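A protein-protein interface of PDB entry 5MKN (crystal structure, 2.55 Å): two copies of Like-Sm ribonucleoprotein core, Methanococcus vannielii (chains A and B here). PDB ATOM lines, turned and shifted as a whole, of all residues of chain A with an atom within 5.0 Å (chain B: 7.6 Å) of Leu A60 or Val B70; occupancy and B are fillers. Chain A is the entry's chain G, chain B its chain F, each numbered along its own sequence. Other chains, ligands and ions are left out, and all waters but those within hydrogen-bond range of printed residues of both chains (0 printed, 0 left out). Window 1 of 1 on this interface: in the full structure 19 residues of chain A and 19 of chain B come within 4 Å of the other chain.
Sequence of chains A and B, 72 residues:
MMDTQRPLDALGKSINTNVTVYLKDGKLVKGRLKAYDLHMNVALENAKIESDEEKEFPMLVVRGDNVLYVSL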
ATOM      1  N   VAL A  29     -35.200  18.422   6.889  1.00  0.00           N
ATOM      2  CA  VAL A  29     -34.194  19.217   7.586  1.00  0.00           C
ATOM      3  C   VAL A  29     -33.164  19.632   6.553  1.00  0.00           C
ATOM      4  O   VAL A  29     -32.532  18.772   5.926  1.00  0.00           O
ATOM      5  CB  VAL A  29     -33.517  18.437   8.730  1.00  0.00           C
ATOM      6  CG1 VAL A  29     -32.648  19.355   9.560  1.00  0.00           C
ATOM      7  CG2 VAL A  29     -34.546  17.743   9.605  1.00  0.00           C
ATOM      8  N   VAL A  42     -25.742  12.660  10.813  1.00  0.00           N
ATOM      9  CA  VAL A  42     -25.231  13.896  10.237  1.00  0.00           C
ATOM     10  C   VAL A  42     -25.276  15.002  11.274  1.00  0.00           C
ATOM     11  O   VAL A  42     -26.145  15.031  12.150  1.00  0.00           O
ATOM     12  CB  VAL A  42     -26.006  14.345   8.976  1.00  0.00           C
ATOM     13  CG1 VAL A  42     -25.809  13.360   7.820  1.00  0.00           C
ATOM     14  CG2 VAL A  42     -27.477  14.548   9.307  1.00  0.00           C
ATOM     15  N   ALA A  43     -24.326  15.922  11.157  1.00  0.00           N
ATOM     16  CA  ALA A  43     -24.390  17.219  11.811  1.00  0.00           C
ATOM     17  C   ALA A  43     -24.724  18.272  10.761  1.00  0.00           C
ATOM     18  O   ALA A  43     -24.202  18.233   9.641  1.00  0.00           O
ATOM     19  CB  ALA A  43     -23.066  17.561  12.507  1.00  0.00           C
ATOM     20  N   LEU A  44     -25.600  19.203  11.117  1.00  0.00           N
ATOM     21  CA  LEU A  44     -26.064  20.216  10.176  1.00  0.00           C
ATOM     22  C   LEU A  44     -25.920  21.598  10.791  1.00  0.00           C
ATOM     23  O   LEU A  44     -26.399  21.842  11.905  1.00  0.00           O
ATOM     24  CB  LEU A  44     -27.517  19.967   9.763  1.00  0.00           C
ATOM     25  CG  LEU A  44     -27.741  18.767   8.841  1.00  0.00           C
ATOM     26  CD1 LEU A  44     -29.222  18.578   8.579  1.00  0.00           C
ATOM     27  CD2 LEU A  44     -26.971  18.941   7.541  1.00  0.00           C
ATOM     28  N   ALA A  47     -29.501  24.803  10.842  1.00  0.00           N
ATOM     29  CA  ALA A  47     -30.525  23.932  10.279  1.00  0.00           C
ATOM     30  C   ALA A  47     -31.923  24.483  10.531  1.00  0.00           C
ATOM     31  O   ALA A  47     -32.183  25.157  11.536  1.00  0.00           O
ATOM     32  CB  ALA A  47     -30.411  22.522  10.860  1.00  0.00           C
ATOM     33  N   ILE A  49     -36.197  23.251   9.940  1.00  0.00           N
ATOM     34  CA  ILE A  49     -37.199  22.261   9.553  1.00  0.00           C
ATOM     35  C   ILE A  49     -38.434  22.982   9.043  1.00  0.00           C
ATOM     36  O   ILE A  49     -39.026  23.810   9.751  1.00  0.00           O
ATOM     37  CB  ILE A  49     -37.556  21.317  10.710  1.00  0.00           C
ATOM     38  CG1 ILE A  49     -36.313  20.583  11.194  1.00  0.00           C
ATOM     39  CG2 ILE A  49     -38.622  20.314  10.285  1.00  0.00           C
ATOM     40  CD1 ILE A  49     -35.807  21.102  12.479  1.00  0.00           C
ATOM     41  N   PHE A  57     -31.745  26.296  14.058  1.00  0.00           N
ATOM     42  CA  PHE A  57     -30.853  25.662  15.013  1.00  0.00           C
ATOM     43  C   PHE A  57     -29.413  25.882  14.591  1.00  0.00           C
ATOM     44  O   PHE A  57     -29.029  25.454  13.489  1.00  0.00           O
ATOM     45  CB  PHE A  57     -31.155  24.174  15.109  1.00  0.00           C
ATOM     46  CG  PHE A  57     -32.601  23.878  15.336  1.00  0.00           C
ATOM     47  CD1 PHE A  57     -33.118  23.851  16.619  1.00  0.00           C
ATOM     48  CD2 PHE A  57     -33.450  23.651  14.271  1.00  0.00           C
ATOM     49  CE1 PHE A  57     -34.450  23.586  16.839  1.00  0.00           C
ATOM     50  CE2 PHE A  57     -34.781  23.398  14.485  1.00  0.00           C
ATOM     51  CZ  PHE A  57     -35.282  23.356  15.770  1.00  0.00           C
ATOM     52  N   PRO A  58     -28.585  26.527  15.417  1.00  0.00           N
ATOM     53  CA  PRO A  58     -27.189  26.754  15.010  1.00  0.00           C
ATOM     54  C   PRO A  58     -26.451  25.467  14.692  1.00  0.00           C
ATOM     55  O   PRO A  58     -25.579  25.469  13.819  1.00  0.00           O
ATOM     56  CB  PRO A  58     -26.583  27.474  16.223  1.00  0.00           C
ATOM     57  CG  PRO A  58     -27.754  27.922  17.053  1.00  0.00           C
ATOM     58  CD  PRO A  58     -28.829  26.929  16.810  1.00  0.00           C
ATOM     59  N   MET A  59     -26.793  24.366  15.362  1.00  0.00           N
ATOM     60  CA  MET A  59     -26.209  23.063  15.067  1.00  0.00           C
ATOM     61  C   MET A  59     -27.211  21.966  15.413  1.00  0.00           C
ATOM     62  O   MET A  59     -27.731  21.920  16.534  1.00  0.00           O
ATOM     63  CB  MET A  59     -24.902  22.864  15.840  1.00  0.00           C
ATOM     64  CG  MET A  59     -24.130  21.647  15.394  1.00  0.00           C
ATOM     65  SD  MET A  59     -23.780  21.704  13.623  1.00  0.00           S
ATOM     66  CE  MET A  59     -22.435  22.878  13.536  1.00  0.00           C
ATOM     67  N   LEU A  60     -27.458  21.070  14.458  1.00  0.00           N
ATOM     68  CA  LEU A  60     -28.463  20.018  14.603  1.00  0.00           C
ATOM     69  C   LEU A  60     -27.836  18.668  14.287  1.00  0.00           C
ATOM     70  O   LEU A  60     -27.460  18.409  13.137  1.00  0.00           O
ATOM     71  CB  LEU A  60     -29.656  20.274  13.684  1.00  0.00           C
ATOM     72  CG  LEU A  60     -30.942  19.698  14.247  1.00  0.00           C
ATOM     73  CD1 LEU A  60     -31.440  20.594  15.373  1.00  0.00           C
ATOM     74  CD2 LEU A  60     -31.990  19.503  13.155  1.00  0.00           C
ATOM     75  N   VAL A  61     -27.739  17.798  15.286  1.00  0.00           N
ATOM     76  CA  VAL A  61     -27.229  16.448  15.080  1.00  0.00           C
ATOM     77  C   VAL A  61     -28.412  15.507  14.895  1.00  0.00           C
ATOM     78  O   VAL A  61     -29.266  15.379  15.787  1.00  0.00           O
ATOM     79  CB  VAL A  61     -26.332  15.990  16.240  1.00  0.00           C
ATOM     80  CG1 VAL A  61     -25.739  14.631  15.907  1.00  0.00           C
ATOM     81  CG2 VAL A  61     -25.229  17.010  16.486  1.00  0.00           C
ATOM     82  N   VAL A  62     -28.448  14.840  13.743  1.00  0.00           N
ATOM     83  CA  VAL A  62     -29.556  13.982  13.344  1.00  0.00           C
ATOM     84  C   VAL A  62     -29.111  12.529  13.449  1.00  0.00           C
ATOM     85  O   VAL A  62     -28.079  12.146  12.883  1.00  0.00           O
ATOM     86  CB  VAL A  62     -30.030  14.300  11.914  1.00  0.00           C
ATOM     87  CG1 VAL A  62     -31.032  13.253  11.448  1.00  0.00           C
ATOM     88  CG2 VAL A  62     -30.598  15.719  11.834  1.00  0.00           C
ATOM     89  N   PRO B   7     -19.725  13.017  13.501  1.00  0.00           N
ATOM     90  CA  PRO B   7     -20.732  14.049  13.797  1.00  0.00           C
ATOM     91  C   PRO B   7     -21.082  14.150  15.270  1.00  0.00           C
ATOM     92  O   PRO B   7     -21.361  15.249  15.753  1.00  0.00           O
ATOM     93  CB  PRO B   7     -21.936  13.610  12.950  1.00  0.00           C
ATOM     94  CG  PRO B   7     -21.766  12.160  12.797  1.00  0.00           C
ATOM     95  CD  PRO B   7     -20.281  11.949  12.657  1.00  0.00           C
ATOM     96  N   LEU B   8     -21.052  13.047  16.013  1.00  0.00           N
ATOM     97  CA  LEU B   8     -21.375  13.159  17.431  1.00  0.00           C
ATOM     98  C   LEU B   8     -20.297  13.862  18.250  1.00  0.00           C
ATOM     99  O   LEU B   8     -20.503  14.052  19.451  1.00  0.00           O
ATOM    100  CB  LEU B   8     -21.656  11.787  18.020  1.00  0.00           C
ATOM    101  CG  LEU B   8     -22.529  10.920  17.125  1.00  0.00           C
ATOM    102  CD1 LEU B   8     -22.569   9.524  17.718  1.00  0.00           C
ATOM    103  CD2 LEU B   8     -23.921  11.518  16.942  1.00  0.00           C
ATOM    104  N   ALA B  10     -20.013  16.896  17.863  1.00  0.00           N
ATOM    105  CA  ALA B  10     -20.755  18.117  18.152  1.00  0.00           C
ATOM    106  C   ALA B  10     -21.425  18.046  19.515  1.00  0.00           C
ATOM    107  O   ALA B  10     -21.598  19.069  20.178  1.00  0.00           O
ATOM    108  CB  ALA B  10     -21.789  18.378  17.059  1.00  0.00           C
ATOM    109  N   LEU B  11     -21.794  16.848  19.967  1.00  0.00           N
ATOM    110  CA  LEU B  11     -22.332  16.737  21.320  1.00  0.00           C
ATOM    111  C   LEU B  11     -21.238  16.809  22.374  1.00  0.00           C
ATOM    112  O   LEU B  11     -21.481  17.283  23.494  1.00  0.00           O
ATOM    113  CB  LEU B  11     -23.119  15.445  21.501  1.00  0.00           C
ATOM    114  CG  LEU B  11     -24.425  15.331  20.709  1.00  0.00           C
ATOM    115  CD1 LEU B  11     -24.220  15.069  19.206  1.00  0.00           C
ATOM    116  CD2 LEU B  11     -25.333  14.300  21.367  1.00  0.00           C
ATOM    117  N   VAL B  19     -29.361  21.997  25.951  1.00  0.00           N
ATOM    118  CA  VAL B  19     -29.704  21.358  24.685  1.00  0.00           C
ATOM    119  C   VAL B  19     -31.164  20.907  24.692  1.00  0.00           C
ATOM    120  O   VAL B  19     -31.811  20.796  25.738  1.00  0.00           O
ATOM    121  CB  VAL B  19     -28.781  20.157  24.383  1.00  0.00           C
ATOM    122  CG1 VAL B  19     -27.332  20.597  24.346  1.00  0.00           C
ATOM    123  CG2 VAL B  19     -28.978  19.066  25.427  1.00  0.00           C
ATOM    124  N   THR B  20     -31.680  20.638  23.496  1.00  0.00           N
ATOM    125  CA  THR B  20     -33.048  20.161  23.322  1.00  0.00           C
ATOM    126  C   THR B  20     -33.017  18.871  22.526  1.00  0.00           C
ATOM    127  O   THR B  20     -32.502  18.847  21.404  1.00  0.00           O
ATOM    128  CB  THR B  20     -33.918  21.202  22.614  1.00  0.00           C
ATOM    129  OG1 THR B  20     -34.005  22.379  23.421  1.00  0.00           O
ATOM    130  CG2 THR B  20     -35.318  20.649  22.389  1.00  0.00           C
ATOM    131  N   VAL B  21     -33.565  17.805  23.099  1.00  0.00           N
ATOM    132  CA  VAL B  21     -33.572  16.492  22.462  1.00  0.00           C
ATOM    133  C   VAL B  21     -34.950  16.236  21.868  1.00  0.00           C
ATOM    134  O   VAL B  21     -35.957  16.269  22.582  1.00  0.00           O
ATOM    135  CB  VAL B  21     -33.185  15.382  23.453  1.00  0.00           C
ATOM    136  CG1 VAL B  21     -33.335  14.020  22.796  1.00  0.00           C
ATOM    137  CG2 VAL B  21     -31.772  15.576  23.934  1.00  0.00           C
ATOM    138  N   TYR B  22     -34.995  15.966  20.569  1.00  0.00           N
ATOM    139  CA  TYR B  22     -36.232  15.659  19.853  1.00  0.00           C
ATOM    140  C   TYR B  22     -36.364  14.146  19.717  1.00  0.00           C
ATOM    141  O   TYR B  22     -35.499  13.497  19.113  1.00  0.00           O
ATOM    142  CB  TYR B  22     -36.243  16.315  18.468  1.00  0.00           C
ATOM    143  CG  TYR B  22     -36.369  17.824  18.481  1.00  0.00           C
ATOM    144  CD1 TYR B  22     -35.352  18.631  18.988  1.00  0.00           C
ATOM    145  CD2 TYR B  22     -37.507  18.448  17.968  1.00  0.00           C
ATOM    146  CE1 TYR B  22     -35.474  20.017  18.996  1.00  0.00           C
ATOM    147  CE2 TYR B  22     -37.643  19.830  17.984  1.00  0.00           C
ATOM    148  CZ  TYR B  22     -36.626  20.605  18.495  1.00  0.00           C
ATOM    149  OH  TYR B  22     -36.768  21.969  18.496  1.00  0.00           O
ATOM    150  N   LEU B  23     -37.428  13.584  20.277  1.00  0.00           N
ATOM    151  CA  LEU B  23     -37.691  12.159  20.156  1.00  0.00           C
ATOM    152  C   LEU B  23     -38.694  11.871  19.040  1.00  0.00           C
ATOM    153  O   LEU B  23     -39.454  12.741  18.603  1.00  0.00           O
ATOM    154  CB  LEU B  23     -38.203  11.573  21.479  1.00  0.00           C
ATOM    155  CG  LEU B  23     -37.535  12.067  22.757  1.00  0.00           C
ATOM    156  CD1 LEU B  23     -38.369  11.660  23.952  1.00  0.00           C
ATOM    157  CD2 LEU B  23     -36.102  11.530  22.860  1.00  0.00           C
ATOM    158  N   VAL B  29     -37.332  17.082  24.894  1.00  0.00           N
ATOM    159  CA  VAL B  29     -36.643  16.935  26.171  1.00  0.00           C
ATOM    160  C   VAL B  29     -35.520  17.960  26.203  1.00  0.00           C
ATOM    161  O   VAL B  29     -34.640  17.961  25.328  1.00  0.00           O
ATOM    162  CB  VAL B  29     -36.113  15.509  26.376  1.00  0.00           C
ATOM    163  CG1 VAL B  29     -35.708  15.310  27.815  1.00  0.00           C
ATOM    164  CG2 VAL B  29     -37.165  14.489  25.970  1.00  0.00           C
ATOM    165  N   LEU B  33     -26.766  18.875  28.897  1.00  0.00           N
ATOM    166  CA  LEU B  33     -26.106  17.667  28.415  1.00  0.00           C
ATOM    167  C   LEU B  33     -24.926  17.313  29.322  1.00  0.00           C
ATOM    168  O   LEU B  33     -23.911  18.015  29.341  1.00  0.00           O
ATOM    169  CB  LEU B  33     -25.655  17.881  26.976  1.00  0.00           C
ATOM    170  CG  LEU B  33     -24.808  16.769  26.365  1.00  0.00           C
ATOM    171  CD1 LEU B  33     -25.548  15.446  26.452  1.00  0.00           C
ATOM    172  CD2 LEU B  33     -24.406  17.114  24.915  1.00  0.00           C
ATOM    173  N   MET B  40     -25.891   7.376  20.898  1.00  0.00           N
ATOM    174  CA  MET B  40     -26.659   8.609  21.059  1.00  0.00           C
ATOM    175  C   MET B  40     -27.539   8.600  22.306  1.00  0.00           C
ATOM    176  O   MET B  40     -28.463   9.416  22.409  1.00  0.00           O
ATOM    177  CB  MET B  40     -27.504   8.924  19.816  1.00  0.00           C
ATOM    178  CG  MET B  40     -26.676   9.159  18.547  1.00  0.00           C
ATOM    179  SD  MET B  40     -27.493  10.205  17.302  1.00  0.00           S
ATOM    180  CE  MET B  40     -27.998  11.575  18.347  1.00  0.00           C
ATOM    181  N   VAL B  42     -28.024   9.901  25.969  1.00  0.00           N
ATOM    182  CA  VAL B  42     -27.626  11.182  26.542  1.00  0.00           C
ATOM    183  C   VAL B  42     -28.144  11.264  27.968  1.00  0.00           C
ATOM    184  O   VAL B  42     -29.287  10.890  28.256  1.00  0.00           O
ATOM    185  CB  VAL B  42     -28.132  12.408  25.730  1.00  0.00           C
ATOM    186  CG1 VAL B  42     -27.524  12.455  24.349  1.00  0.00           C
ATOM    187  CG2 VAL B  42     -29.644  12.460  25.677  1.00  0.00           C
ATOM    188  N   VAL B  67     -34.151   8.855  19.649  1.00  0.00           N
ATOM    189  CA  VAL B  67     -33.788  10.231  19.330  1.00  0.00           C
ATOM    190  C   VAL B  67     -34.038  10.496  17.855  1.00  0.00           C
ATOM    191  O   VAL B  67     -33.632   9.706  16.988  1.00  0.00           O
ATOM    192  CB  VAL B  67     -32.323  10.514  19.694  1.00  0.00           C
ATOM    193  CG1 VAL B  67     -31.823  11.772  18.968  1.00  0.00           C
ATOM    194  CG2 VAL B  67     -32.184  10.654  21.191  1.00  0.00           C
ATOM    195  N   LEU B  68     -34.706  11.613  17.572  1.00  0.00           N
ATOM    196  CA  LEU B  68     -34.857  12.094  16.205  1.00  0.00           C
ATOM    197  C   LEU B  68     -33.662  12.963  15.823  1.00  0.00           C
ATOM    198  O   LEU B  68     -32.890  12.611  14.921  1.00  0.00           O
ATOM    199  CB  LEU B  68     -36.183  12.855  16.073  1.00  0.00           C
ATOM    200  CG  LEU B  68     -36.564  13.438  14.716  1.00  0.00           C
ATOM    201  CD1 LEU B  68     -36.285  12.459  13.612  1.00  0.00           C
ATOM    202  CD2 LEU B  68     -38.042  13.814  14.730  1.00  0.00           C
ATOM    203  N   TYR B  69     -33.500  14.096  16.513  1.00  0.00           N
ATOM    204  CA  TYR B  69     -32.308  14.920  16.402  1.00  0.00           C
ATOM    205  C   TYR B  69     -32.113  15.680  17.706  1.00  0.00           C
ATOM    206  O   TYR B  69     -33.038  15.840  18.511  1.00  0.00           O
ATOM    207  CB  TYR B  69     -32.352  15.895  15.205  1.00  0.00           C
ATOM    208  CG  TYR B  69     -33.683  16.585  14.938  1.00  0.00           C
ATOM    209  CD1 TYR B  69     -34.116  17.653  15.716  1.00  0.00           C
ATOM    210  CD2 TYR B  69     -34.490  16.186  13.878  1.00  0.00           C
ATOM    211  CE1 TYR B  69     -35.329  18.293  15.449  1.00  0.00           C
ATOM    212  CE2 TYR B  69     -35.696  16.817  13.608  1.00  0.00           C
ATOM    213  CZ  TYR B  69     -36.112  17.863  14.395  1.00  0.00           C
ATOM    214  OH  TYR B  69     -37.317  18.472  14.118  1.00  0.00           O
ATOM    215  N   VAL B  70     -30.880  16.126  17.923  1.00  0.00           N
ATOM    216  CA  VAL B  70     -30.538  16.905  19.105  1.00  0.00           C
ATOM    217  C   VAL B  70     -30.076  18.278  18.644  1.00  0.00           C
ATOM    218  O   VAL B  70     -29.277  18.394  17.707  1.00  0.00           O
ATOM    219  CB  VAL B  70     -29.488  16.196  19.985  1.00  0.00           C
ATOM    220  CG1 VAL B  70     -29.866  14.728  20.141  1.00  0.00           C
ATOM    221  CG2 VAL B  70     -28.064  16.335  19.434  1.00  0.00           C
ATOM    222  N   SER B  71     -30.636  19.310  19.262  1.00  0.00           N
ATOM    223  CA  SER B  71     -30.401  20.694  18.879  1.00  0.00           C
ATOM    224  C   SER B  71     -29.350  21.314  19.793  1.00  0.00           C
ATOM    225  O   SER B  71     -29.450  21.209  21.023  1.00  0.00           O
ATOM    226  CB  SER B  71     -31.701  21.493  18.946  1.00  0.00           C
ATOM    227  OG  SER B  71     -31.430  22.877  19.022  1.00  0.00           O
ATOM    228  N   LEU B  72     -28.352  21.962  19.186  1.00  0.00           N
ATOM    229  CA  LEU B  72     -27.263  22.599  19.934  1.00  0.00           C
ATOM    230  C   LEU B  72     -27.177  24.102  19.661  1.00  0.00           C
ATOM    231  O   LEU B  72     -26.121  24.724  19.832  1.00  0.00           O
ATOM    232  CB  LEU B  72     -25.925  21.934  19.600  1.00  0.00           C
ATOM    233  CG  LEU B  72     -25.944  20.407  19.616  1.00  0.00           C
ATOM    234  CD1 LEU B  72     -24.584  19.845  19.265  1.00  0.00           C
ATOM    235  CD2 LEU B  72     -26.402  19.926  20.976  1.00  0.00           C
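N of Val B70 lies within hydrogen-bond range of O of Val A61. N of Leu B72 is in hydrogen-bond range of O of Met A59, 2.7 Å away.
The backbone carbonyl oxygen (O) of Thr B20 is in hydrogen-bond range of the backbone NH (N) of Ser B71 (2.9 Å). The backbone NH of Leu B68 is in hydrogen-bond range of the backbone carbonyl oxygen of Tyr B22 (2.6 Å). N of Tyr B22 lies within hydrogen-bond range of O of Tyr B69 (2.8 Å). N of Val A62 lies within hydrogen-bond range of O of Val A42 (2.8 Å). The backbone NH (N) of Leu A44 is in hydrogen-bond range of the backbone carbonyl oxygen (O) of Leu A60 (2.9 Å). N of Ala A47 sits at hydrogen-bond distance from O of Phe A57 (2.8 Å).
Phe A57 touches Tyr B22 (CE1 to OH, 3.3 Å). CD1 of Phe A57 touches OG of Ser B71 (3.1 Å). Ser B71 touches Met A59 (C to O, 3.7 Å). Leu A60 touches Tyr B69 (CD2 to CD1, 3.8 Å). CA of Leu A60 touches O of Val B70 (3.6 Å). Leu A60 touches Ser B71 (CD1 to CA, 3.7 Å). Ala B10 touches Val A61. CG2 of Val A61 touches CD1 of Leu B11, 3.5 Å away. CA of Tyr B69 touches O of Val A61, 3.1 Å away. Leu B68 touches Val A62 (O to CA, 3.9 Å).
Printed residues of chain B within 4 Å of Val A42: Pro B7. Leu A60 touches just these residues of chain B: Tyr B69, Val B70 and Ser B71. Printed residues of chain A within 4 Å of Pro B7: Val A42 (3.99 Å) and Ala A43 (3.8 Å). Val B70 touches just these residues of chain A: Leu A60 and Val A61. The nearest residue of chain B that does not touch Leu A60 is Leu B72 (4.9 Å). The nearest residue of chain A that does not touch Val B70 is Met A59 (4.02 Å).
Printed residues of chain A that touch a printed residue of chain B: Val A42, Ala A43, Ile A49, Phe A57, Met A59, Leu A60, Val A61 and Val A62.
Positions printed for both chains: 29 and 42. Of the 17 pairs that touch across the chains among the printed residues, none has its exchanged pair printed and touching as well.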
